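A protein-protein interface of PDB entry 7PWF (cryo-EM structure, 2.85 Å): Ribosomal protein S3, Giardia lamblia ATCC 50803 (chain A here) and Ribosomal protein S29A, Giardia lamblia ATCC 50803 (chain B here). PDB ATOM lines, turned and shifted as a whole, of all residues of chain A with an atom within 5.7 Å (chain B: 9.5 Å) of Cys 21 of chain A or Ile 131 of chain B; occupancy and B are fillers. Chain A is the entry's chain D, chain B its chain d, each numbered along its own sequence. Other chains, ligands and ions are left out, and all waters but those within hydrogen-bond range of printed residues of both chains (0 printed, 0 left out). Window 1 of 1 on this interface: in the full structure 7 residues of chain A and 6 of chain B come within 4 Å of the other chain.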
ATOM      1  N   LYS A  16     -15.320  -4.557  12.288  1.00  0.00           N
ATOM      2  CA  LYS A  16     -15.510  -5.839  11.627  1.00  0.00           C
ATOM      3  C   LYS A  16     -16.330  -5.661  10.354  1.00  0.00           C
ATOM      4  O   LYS A  16     -15.961  -6.160   9.283  1.00  0.00           O
ATOM      5  CB  LYS A  16     -16.210  -6.806  12.591  1.00  0.00           C
ATOM      6  CG  LYS A  16     -15.803  -8.262  12.480  1.00  0.00           C
ATOM      7  CD  LYS A  16     -14.407  -8.501  13.040  1.00  0.00           C
ATOM      8  CE  LYS A  16     -14.181  -9.974  13.358  1.00  0.00           C
ATOM      9  NZ  LYS A  16     -14.021 -10.801  12.131  1.00  0.00           N
ATOM     10  N   TYR A  17     -17.434  -4.921  10.463  1.00  0.00           N
ATOM     11  CA  TYR A  17     -18.306  -4.727   9.316  1.00  0.00           C
ATOM     12  C   TYR A  17     -17.625  -3.898   8.239  1.00  0.00           C
ATOM     13  O   TYR A  17     -17.862  -4.125   7.047  1.00  0.00           O
ATOM     14  CB  TYR A  17     -19.613  -4.063   9.749  1.00  0.00           C
ATOM     15  CG  TYR A  17     -20.686  -4.133   8.694  1.00  0.00           C
ATOM     16  CD1 TYR A  17     -21.007  -5.341   8.087  1.00  0.00           C
ATOM     17  CD2 TYR A  17     -21.365  -2.999   8.286  1.00  0.00           C
ATOM     18  CE1 TYR A  17     -21.981  -5.415   7.119  1.00  0.00           C
ATOM     19  CE2 TYR A  17     -22.332  -3.062   7.316  1.00  0.00           C
ATOM     20  CZ  TYR A  17     -22.637  -4.269   6.736  1.00  0.00           C
ATOM     21  OH  TYR A  17     -23.609  -4.334   5.766  1.00  0.00           O
ATOM     22  N   LEU A  18     -16.768  -2.949   8.625  1.00  0.00           N
ATOM     23  CA  LEU A  18     -16.065  -2.166   7.615  1.00  0.00           C
ATOM     24  C   LEU A  18     -15.109  -3.035   6.805  1.00  0.00           C
ATOM     25  O   LEU A  18     -15.011  -2.889   5.580  1.00  0.00           O
ATOM     26  CB  LEU A  18     -15.323  -1.001   8.266  1.00  0.00           C
ATOM     27  CG  LEU A  18     -14.566  -0.068   7.317  1.00  0.00           C
ATOM     28  CD1 LEU A  18     -15.527   0.806   6.539  1.00  0.00           C
ATOM     29  CD2 LEU A  18     -13.593   0.798   8.088  1.00  0.00           C
ATOM     30  N   ASN A  19     -14.407  -3.957   7.466  1.00  0.00           N
ATOM     31  CA  ASN A  19     -13.495  -4.834   6.739  1.00  0.00           C
ATOM     32  C   ASN A  19     -14.246  -5.824   5.863  1.00  0.00           C
ATOM     33  O   ASN A  19     -13.784  -6.142   4.763  1.00  0.00           O
ATOM     34  CB  ASN A  19     -12.577  -5.565   7.713  1.00  0.00           C
ATOM     35  CG  ASN A  19     -11.345  -4.758   8.063  1.00  0.00           C
ATOM     36  OD1 ASN A  19     -11.232  -4.232   9.165  1.00  0.00           O
ATOM     37  ND2 ASN A  19     -10.417  -4.656   7.123  1.00  0.00           N
ATOM     38  N   ASP A  20     -15.407  -6.311   6.313  1.00  0.00           N
ATOM     39  CA  ASP A  20     -16.253  -7.078   5.397  1.00  0.00           C
ATOM     40  C   ASP A  20     -16.666  -6.243   4.189  1.00  0.00           C
ATOM     41  O   ASP A  20     -16.694  -6.746   3.058  1.00  0.00           O
ATOM     42  CB  ASP A  20     -17.490  -7.634   6.111  1.00  0.00           C
ATOM     43  CG  ASP A  20     -17.156  -8.709   7.136  1.00  0.00           C
ATOM     44  OD1 ASP A  20     -16.702  -8.394   8.251  1.00  0.00           O
ATOM     45  OD2 ASP A  20     -17.358  -9.894   6.817  1.00  0.00           O
ATOM     46  N   CYS A  21     -16.988  -4.967   4.410  1.00  0.00           N
ATOM     47  CA  CYS A  21     -17.398  -4.099   3.309  1.00  0.00           C
ATOM     48  C   CYS A  21     -16.279  -3.925   2.288  1.00  0.00           C
ATOM     49  O   CYS A  21     -16.531  -3.909   1.079  1.00  0.00           O
ATOM     50  CB  CYS A  21     -17.834  -2.741   3.857  1.00  0.00           C
ATOM     51  SG  CYS A  21     -19.551  -2.659   4.386  1.00  0.00           S
ATOM     52  N   ILE A  22     -15.042  -3.771   2.755  1.00  0.00           N
ATOM     53  CA  ILE A  22     -13.912  -3.603   1.841  1.00  0.00           C
ATOM     54  C   ILE A  22     -13.575  -4.915   1.129  1.00  0.00           C
ATOM     55  O   ILE A  22     -13.236  -4.927  -0.066  1.00  0.00           O
ATOM     56  CB  ILE A  22     -12.701  -3.036   2.604  1.00  0.00           C
ATOM     57  CG1 ILE A  22     -13.032  -1.657   3.170  1.00  0.00           C
ATOM     58  CG2 ILE A  22     -11.499  -2.931   1.697  1.00  0.00           C
ATOM     59  CD1 ILE A  22     -12.408  -1.379   4.506  1.00  0.00           C
ATOM     60  N   MET A  23     -13.665  -6.038   1.845  1.00  0.00           N
ATOM     61  CA  MET A  23     -13.398  -7.337   1.238  1.00  0.00           C
ATOM     62  C   MET A  23     -14.419  -7.672   0.155  1.00  0.00           C
ATOM     63  O   MET A  23     -14.076  -8.313  -0.843  1.00  0.00           O
ATOM     64  CB  MET A  23     -13.382  -8.407   2.331  1.00  0.00           C
ATOM     65  CG  MET A  23     -13.320  -9.842   1.848  1.00  0.00           C
ATOM     66  SD  MET A  23     -13.747 -11.002   3.167  1.00  0.00           S
ATOM     67  CE  MET A  23     -14.246 -12.432   2.220  1.00  0.00           C
ATOM     68  N   GLU A  24     -15.670  -7.241   0.331  1.00  0.00           N
ATOM     69  CA  GLU A  24     -16.669  -7.430  -0.713  1.00  0.00           C
ATOM     70  C   GLU A  24     -16.264  -6.735  -2.007  1.00  0.00           C
ATOM     71  O   GLU A  24     -16.465  -7.284  -3.099  1.00  0.00           O
ATOM     72  CB  GLU A  24     -18.027  -6.922  -0.222  1.00  0.00           C
ATOM     73  CG  GLU A  24     -19.228  -7.491  -0.950  1.00  0.00           C
ATOM     74  CD  GLU A  24     -20.535  -7.236  -0.213  1.00  0.00           C
ATOM     75  OE1 GLU A  24     -21.547  -6.922  -0.872  1.00  0.00           O
ATOM     76  OE2 GLU A  24     -20.553  -7.341   1.031  1.00  0.00           O
ATOM     77  N   ALA A  25     -15.668  -5.543  -1.911  1.00  0.00           N
ATOM     78  CA  ALA A  25     -15.231  -4.829  -3.108  1.00  0.00           C
ATOM     79  C   ALA A  25     -14.019  -5.495  -3.742  1.00  0.00           C
ATOM     80  O   ALA A  25     -13.918  -5.570  -4.976  1.00  0.00           O
ATOM     81  CB  ALA A  25     -14.925  -3.374  -2.768  1.00  0.00           C
ATOM     82  N   GLU A  26     -13.095  -5.986  -2.911  1.00  0.00           N
ATOM     83  CA  GLU A  26     -12.006  -6.819  -3.421  1.00  0.00           C
ATOM     84  C   GLU A  26     -12.541  -7.984  -4.256  1.00  0.00           C
ATOM     85  O   GLU A  26     -12.102  -8.213  -5.395  1.00  0.00           O
ATOM     86  CB  GLU A  26     -11.170  -7.341  -2.250  1.00  0.00           C
ATOM     87  CG  GLU A  26      -9.985  -8.213  -2.640  1.00  0.00           C
ATOM     88  CD  GLU A  26      -8.728  -7.439  -2.967  1.00  0.00           C
ATOM     89  OE1 GLU A  26      -8.344  -7.413  -4.151  1.00  0.00           O
ATOM     90  OE2 GLU A  26      -8.108  -6.888  -2.035  1.00  0.00           O
ATOM     91  N   CYS B 102      -1.760   2.924  -1.085  1.00  0.00           N
ATOM     92  CA  CYS B 102      -3.180   2.692  -1.293  1.00  0.00           C
ATOM     93  C   CYS B 102      -3.435   1.202  -1.481  1.00  0.00           C
ATOM     94  O   CYS B 102      -2.698   0.524  -2.203  1.00  0.00           O
ATOM     95  CB  CYS B 102      -3.684   3.481  -2.500  1.00  0.00           C
ATOM     96  SG  CYS B 102      -5.293   2.967  -3.134  1.00  0.00           S
ATOM     97  N   ARG B 103      -4.479   0.696  -0.823  1.00  0.00           N
ATOM     98  CA  ARG B 103      -4.831  -0.716  -0.928  1.00  0.00           C
ATOM     99  C   ARG B 103      -5.200  -1.129  -2.346  1.00  0.00           C
ATOM    100  O   ARG B 103      -5.155  -2.322  -2.659  1.00  0.00           O
ATOM    101  CB  ARG B 103      -5.992  -1.046   0.018  1.00  0.00           C
ATOM    102  CG  ARG B 103      -5.576  -1.149   1.461  1.00  0.00           C
ATOM    103  CD  ARG B 103      -6.414  -2.130   2.249  1.00  0.00           C
ATOM    104  NE  ARG B 103      -7.448  -1.478   3.043  1.00  0.00           N
ATOM    105  CZ  ARG B 103      -8.171  -2.099   3.970  1.00  0.00           C
ATOM    106  NH1 ARG B 103      -7.979  -3.388   4.210  1.00  0.00           N
ATOM    107  NH2 ARG B 103      -9.080  -1.432   4.664  1.00  0.00           N
ATOM    108  N   ILE B 104      -5.559  -0.188  -3.209  1.00  0.00           N
ATOM    109  CA  ILE B 104      -6.094  -0.497  -4.525  1.00  0.00           C
ATOM    110  C   ILE B 104      -5.069  -0.238  -5.631  1.00  0.00           C
ATOM    111  O   ILE B 104      -4.862  -1.087  -6.497  1.00  0.00           O
ATOM    112  CB  ILE B 104      -7.405   0.278  -4.780  1.00  0.00           C
ATOM    113  CG1 ILE B 104      -8.524  -0.308  -3.926  1.00  0.00           C
ATOM    114  CG2 ILE B 104      -7.807   0.168  -6.231  1.00  0.00           C
ATOM    115  CD1 ILE B 104      -9.730   0.574  -3.801  1.00  0.00           C
ATOM    116  N   TYR B 115     -10.680   5.637  10.189  1.00  0.00           N
ATOM    117  CA  TYR B 115     -11.480   4.417  10.287  1.00  0.00           C
ATOM    118  C   TYR B 115     -10.712   3.176   9.844  1.00  0.00           C
ATOM    119  O   TYR B 115     -11.255   2.068   9.889  1.00  0.00           O
ATOM    120  CB  TYR B 115     -12.770   4.514   9.463  1.00  0.00           C
ATOM    121  CG  TYR B 115     -13.566   5.784   9.615  1.00  0.00           C
ATOM    122  CD1 TYR B 115     -14.062   6.176  10.847  1.00  0.00           C
ATOM    123  CD2 TYR B 115     -13.852   6.575   8.510  1.00  0.00           C
ATOM    124  CE1 TYR B 115     -14.800   7.330  10.980  1.00  0.00           C
ATOM    125  CE2 TYR B 115     -14.594   7.726   8.633  1.00  0.00           C
ATOM    126  CZ  TYR B 115     -15.062   8.101   9.870  1.00  0.00           C
ATOM    127  OH  TYR B 115     -15.795   9.253   9.995  1.00  0.00           O
ATOM    128  N   GLY B 116      -9.456   3.332   9.435  1.00  0.00           N
ATOM    129  CA  GLY B 116      -8.710   2.213   8.895  1.00  0.00           C
ATOM    130  C   GLY B 116      -9.021   1.852   7.458  1.00  0.00           C
ATOM    131  O   GLY B 116      -8.973   0.672   7.103  1.00  0.00           O
ATOM    132  N   LEU B 117      -9.340   2.834   6.612  1.00  0.00           N
ATOM    133  CA  LEU B 117      -9.562   2.553   5.195  1.00  0.00           C
ATOM    134  C   LEU B 117      -8.256   2.240   4.480  1.00  0.00           C
ATOM    135  O   LEU B 117      -8.121   1.186   3.848  1.00  0.00           O
ATOM    136  CB  LEU B 117     -10.285   3.718   4.511  1.00  0.00           C
ATOM    137  CG  LEU B 117     -11.803   3.898   4.653  1.00  0.00           C
ATOM    138  CD1 LEU B 117     -12.556   2.768   3.957  1.00  0.00           C
ATOM    139  CD2 LEU B 117     -12.247   3.984   6.081  1.00  0.00           C
ATOM    140  N   PHE B 118      -7.291   3.158   4.544  1.00  0.00           N
ATOM    141  CA  PHE B 118      -5.978   2.975   3.927  1.00  0.00           C
ATOM    142  C   PHE B 118      -6.079   2.887   2.405  1.00  0.00           C
ATOM    143  O   PHE B 118      -5.451   2.032   1.780  1.00  0.00           O
ATOM    144  CB  PHE B 118      -5.254   1.747   4.496  1.00  0.00           C
ATOM    145  CG  PHE B 118      -4.665   1.967   5.863  1.00  0.00           C
ATOM    146  CD1 PHE B 118      -3.574   2.802   6.037  1.00  0.00           C
ATOM    147  CD2 PHE B 118      -5.201   1.341   6.971  1.00  0.00           C
ATOM    148  CE1 PHE B 118      -3.035   3.007   7.287  1.00  0.00           C
ATOM    149  CE2 PHE B 118      -4.662   1.545   8.227  1.00  0.00           C
ATOM    150  CZ  PHE B 118      -3.580   2.379   8.381  1.00  0.00           C
ATOM    151  N   ILE B 119      -6.874   3.774   1.800  1.00  0.00           N
ATOM    152  CA  ILE B 119      -6.927   3.921   0.353  1.00  0.00           C
ATOM    153  C   ILE B 119      -6.852   5.401   0.009  1.00  0.00           C
ATOM    154  O   ILE B 119      -7.222   6.267   0.802  1.00  0.00           O
ATOM    155  CB  ILE B 119      -8.187   3.274  -0.262  1.00  0.00           C
ATOM    156  CG1 ILE B 119      -9.443   3.678   0.497  1.00  0.00           C
ATOM    157  CG2 ILE B 119      -8.075   1.776  -0.257  1.00  0.00           C
ATOM    158  CD1 ILE B 119     -10.676   2.981  -0.011  1.00  0.00           C
ATOM    159  N   CYS B 120      -6.369   5.685  -1.198  1.00  0.00           N
ATOM    160  CA  CYS B 120      -6.091   7.049  -1.622  1.00  0.00           C
ATOM    161  C   CYS B 120      -7.365   7.761  -2.088  1.00  0.00           C
ATOM    162  O   CYS B 120      -8.422   7.156  -2.277  1.00  0.00           O
ATOM    163  CB  CYS B 120      -5.042   7.059  -2.730  1.00  0.00           C
ATOM    164  SG  CYS B 120      -5.686   6.801  -4.393  1.00  0.00           S
ATOM    165  N   CYS B 123      -8.706   6.798  -5.767  1.00  0.00           N
ATOM    166  CA  CYS B 123      -9.406   5.518  -5.802  1.00  0.00           C
ATOM    167  C   CYS B 123     -10.636   5.500  -4.910  1.00  0.00           C
ATOM    168  O   CYS B 123     -11.512   4.655  -5.109  1.00  0.00           O
ATOM    169  CB  CYS B 123      -8.477   4.370  -5.406  1.00  0.00           C
ATOM    170  SG  CYS B 123      -6.964   4.222  -6.377  1.00  0.00           S
ATOM    171  N   PHE B 124     -10.732   6.407  -3.937  1.00  0.00           N
ATOM    172  CA  PHE B 124     -11.880   6.393  -3.040  1.00  0.00           C
ATOM    173  C   PHE B 124     -13.143   6.882  -3.732  1.00  0.00           C
ATOM    174  O   PHE B 124     -14.243   6.557  -3.281  1.00  0.00           O
ATOM    175  CB  PHE B 124     -11.586   7.236  -1.793  1.00  0.00           C
ATOM    176  CG  PHE B 124     -12.680   7.209  -0.757  1.00  0.00           C
ATOM    177  CD1 PHE B 124     -12.672   6.251   0.245  1.00  0.00           C
ATOM    178  CD2 PHE B 124     -13.705   8.141  -0.772  1.00  0.00           C
ATOM    179  CE1 PHE B 124     -13.670   6.215   1.201  1.00  0.00           C
ATOM    180  CE2 PHE B 124     -14.710   8.106   0.180  1.00  0.00           C
ATOM    181  CZ  PHE B 124     -14.690   7.145   1.166  1.00  0.00           C
ATOM    182  N   LYS B 125     -13.013   7.633  -4.828  1.00  0.00           N
ATOM    183  CA  LYS B 125     -14.186   8.187  -5.496  1.00  0.00           C
ATOM    184  C   LYS B 125     -15.020   7.107  -6.175  1.00  0.00           C
ATOM    185  O   LYS B 125     -16.252   7.142  -6.109  1.00  0.00           O
ATOM    186  CB  LYS B 125     -13.767   9.246  -6.519  1.00  0.00           C
ATOM    187  CG  LYS B 125     -12.741  10.251  -6.035  1.00  0.00           C
ATOM    188  CD  LYS B 125     -12.086  10.960  -7.213  1.00  0.00           C
ATOM    189  CE  LYS B 125     -11.848  12.438  -6.941  1.00  0.00           C
ATOM    190  NZ  LYS B 125     -11.106  12.676  -5.679  1.00  0.00           N
ATOM    191  N   GLU B 126     -14.378   6.145  -6.839  1.00  0.00           N
ATOM    192  CA  GLU B 126     -15.100   5.169  -7.651  1.00  0.00           C
ATOM    193  C   GLU B 126     -15.354   3.846  -6.944  1.00  0.00           C
ATOM    194  O   GLU B 126     -16.347   3.180  -7.251  1.00  0.00           O
ATOM    195  CB  GLU B 126     -14.349   4.896  -8.959  1.00  0.00           C
ATOM    196  CG  GLU B 126     -12.884   4.545  -8.784  1.00  0.00           C
ATOM    197  CD  GLU B 126     -12.007   5.768  -8.674  1.00  0.00           C
ATOM    198  OE1 GLU B 126     -12.439   6.731  -8.016  1.00  0.00           O
ATOM    199  OE2 GLU B 126     -10.887   5.760  -9.224  1.00  0.00           O
ATOM    200  N   ASN B 127     -14.501   3.446  -6.008  1.00  0.00           N
ATOM    201  CA  ASN B 127     -14.778   2.257  -5.216  1.00  0.00           C
ATOM    202  C   ASN B 127     -15.711   2.536  -4.046  1.00  0.00           C
ATOM    203  O   ASN B 127     -16.070   1.601  -3.329  1.00  0.00           O
ATOM    204  CB  ASN B 127     -13.474   1.640  -4.696  1.00  0.00           C
ATOM    205  CG  ASN B 127     -12.494   1.304  -5.809  1.00  0.00           C
ATOM    206  OD1 ASN B 127     -11.832   2.176  -6.357  1.00  0.00           O
ATOM    207  ND2 ASN B 127     -12.397   0.024  -6.136  1.00  0.00           N
ATOM    208  N   ALA B 128     -16.111   3.795  -3.840  1.00  0.00           N
ATOM    209  CA  ALA B 128     -16.970   4.130  -2.711  1.00  0.00           C
ATOM    210  C   ALA B 128     -18.376   3.579  -2.867  1.00  0.00           C
ATOM    211  O   ALA B 128     -19.081   3.440  -1.864  1.00  0.00           O
ATOM    212  CB  ALA B 128     -17.042   5.644  -2.518  1.00  0.00           C
ATOM    213  N   GLY B 129     -18.797   3.266  -4.092  1.00  0.00           N
ATOM    214  CA  GLY B 129     -20.133   2.729  -4.284  1.00  0.00           C
ATOM    215  C   GLY B 129     -20.345   1.413  -3.560  1.00  0.00           C
ATOM    216  O   GLY B 129     -21.330   1.239  -2.840  1.00  0.00           O
ATOM    217  N   LYS B 130     -19.407   0.477  -3.719  1.00  0.00           N
ATOM    218  CA  LYS B 130     -19.564  -0.851  -3.138  1.00  0.00           C
ATOM    219  C   LYS B 130     -18.997  -0.951  -1.730  1.00  0.00           C
ATOM    220  O   LYS B 130     -19.543  -1.691  -0.907  1.00  0.00           O
ATOM    221  CB  LYS B 130     -18.920  -1.910  -4.032  1.00  0.00           C
ATOM    222  CG  LYS B 130     -19.669  -3.236  -4.021  1.00  0.00           C
ATOM    223  CD  LYS B 130     -19.127  -4.204  -5.045  1.00  0.00           C
ATOM    224  CE  LYS B 130     -20.156  -5.273  -5.390  1.00  0.00           C
ATOM    225  NZ  LYS B 130     -20.113  -6.448  -4.477  1.00  0.00           N
ATOM    226  N   ILE B 131     -17.907  -0.235  -1.430  1.00  0.00           N
ATOM    227  CA  ILE B 131     -17.439  -0.158  -0.048  1.00  0.00           C
ATOM    228  C   ILE B 131     -18.579   0.281   0.856  1.00  0.00           C
ATOM    229  O   ILE B 131     -18.757  -0.242   1.961  1.00  0.00           O
ATOM    230  CB  ILE B 131     -16.223   0.780   0.064  1.00  0.00           C
ATOM    231  CG1 ILE B 131     -15.052   0.242  -0.757  1.00  0.00           C
ATOM    232  CG2 ILE B 131     -15.799   0.944   1.505  1.00  0.00           C
ATOM    233  CD1 ILE B 131     -13.870   1.186  -0.801  1.00  0.00           C
ATOM    234  N   GLY B 132     -19.380   1.233   0.394  1.00  0.00           N
ATOM    235  CA  GLY B 132     -20.663   1.475   1.014  1.00  0.00           C
ATOM    236  C   GLY B 132     -21.052   2.930   1.133  1.00  0.00           C
ATOM    237  O   GLY B 132     -22.225   3.242   1.349  1.00  0.00           O
ATOM    238  N   PHE B 133     -20.082   3.828   1.009  1.00  0.00           N
ATOM    239  CA  PHE B 133     -20.366   5.242   1.198  1.00  0.00           C
ATOM    240  C   PHE B 133     -21.283   5.743   0.089  1.00  0.00           C
ATOM    241  O   PHE B 133     -21.149   5.354  -1.074  1.00  0.00           O
ATOM    242  CB  PHE B 133     -19.066   6.043   1.224  1.00  0.00           C
ATOM    243  CG  PHE B 133     -18.193   5.737   2.409  1.00  0.00           C
ATOM    244  CD1 PHE B 133     -17.382   4.618   2.417  1.00  0.00           C
ATOM    245  CD2 PHE B 133     -18.206   6.551   3.526  1.00  0.00           C
ATOM    246  CE1 PHE B 133     -16.589   4.329   3.505  1.00  0.00           C
ATOM    247  CE2 PHE B 133     -17.419   6.263   4.618  1.00  0.00           C
ATOM    248  CZ  PHE B 133     -16.608   5.154   4.608  1.00  0.00           C
ATOM    249  N   VAL B 134     -22.237   6.596   0.458  1.00  0.00           N
ATOM    250  CA  VAL B 134     -23.169   7.177  -0.497  1.00  0.00           C
ATOM    251  C   VAL B 134     -23.409   8.636  -0.127  1.00  0.00           C
ATOM    252  O   VAL B 134     -23.285   9.031   1.035  1.00  0.00           O
ATOM    253  CB  VAL B 134     -24.489   6.364  -0.563  1.00  0.00           C
ATOM    254  CG1 VAL B 134     -25.357   6.610   0.652  1.00  0.00           C
ATOM    255  CG2 VAL B 134     -25.254   6.667  -1.845  1.00  0.00           C
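NZ of Lys 130 of chain B lies within salt-bridge range of OE1 of Glu 24 of chain A (3.9 Å). The side-chain sulfur (SG) of Cys 21 of chain A lies close to the backbone carbonyl oxygen (O) of Ile 131 of chain B.
NH2 of Arg 103 of chain B lies within hydrogen-bond range of O of Gly 116 of chain B, 3.2 Å away. The backbone carbonyl oxygen (O) of Leu 117 of chain B lies within hydrogen-bond range of the guanidinium group (NE) of Arg 103 of chain B (2.9 Å). N of Arg 103 of chain B sits at hydrogen-bond distance from O of Phe 118 of chain B (3.1 Å). The side-chain sulfur of Cys 21 of chain A is in hydrogen-bond range of the backbone carbonyl oxygen of Tyr 17 of chain A, 3.5 Å away.
Leu 18 of chain A touches Tyr 115 of chain B (CD2 to O, 3.2 Å). Leu 18 of chain A touches Leu 117 of chain B. Ile 22 of chain A touches Arg 103 of chain B (CD1 to NH2, 3.3 Å).
Printed residues of chain B within 4 Å of Leu 18 of chain A: Tyr 115 and Leu 117. Of chain B, only Ile 131 (3.3 Å) comes within 4 Å of Cys 21 of chain A. Of the printed residues of chain A, Lys 130 of chain B touches Glu 24. Of chain A, only Cys 21 comes within 4 Å of Ile 131 of chain B.
Printed residues of chain B that touch a printed residue of chain A: Arg 103, Tyr 115, Leu 117, Lys 130 and Ile 131. Among the printed residues, Asp or Glu carboxylates within 4 Å of a Lys or Arg side-chain nitrogen of the other chain: Glu 24 of chain A with Lys 130 of chain B (3.9 Å).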
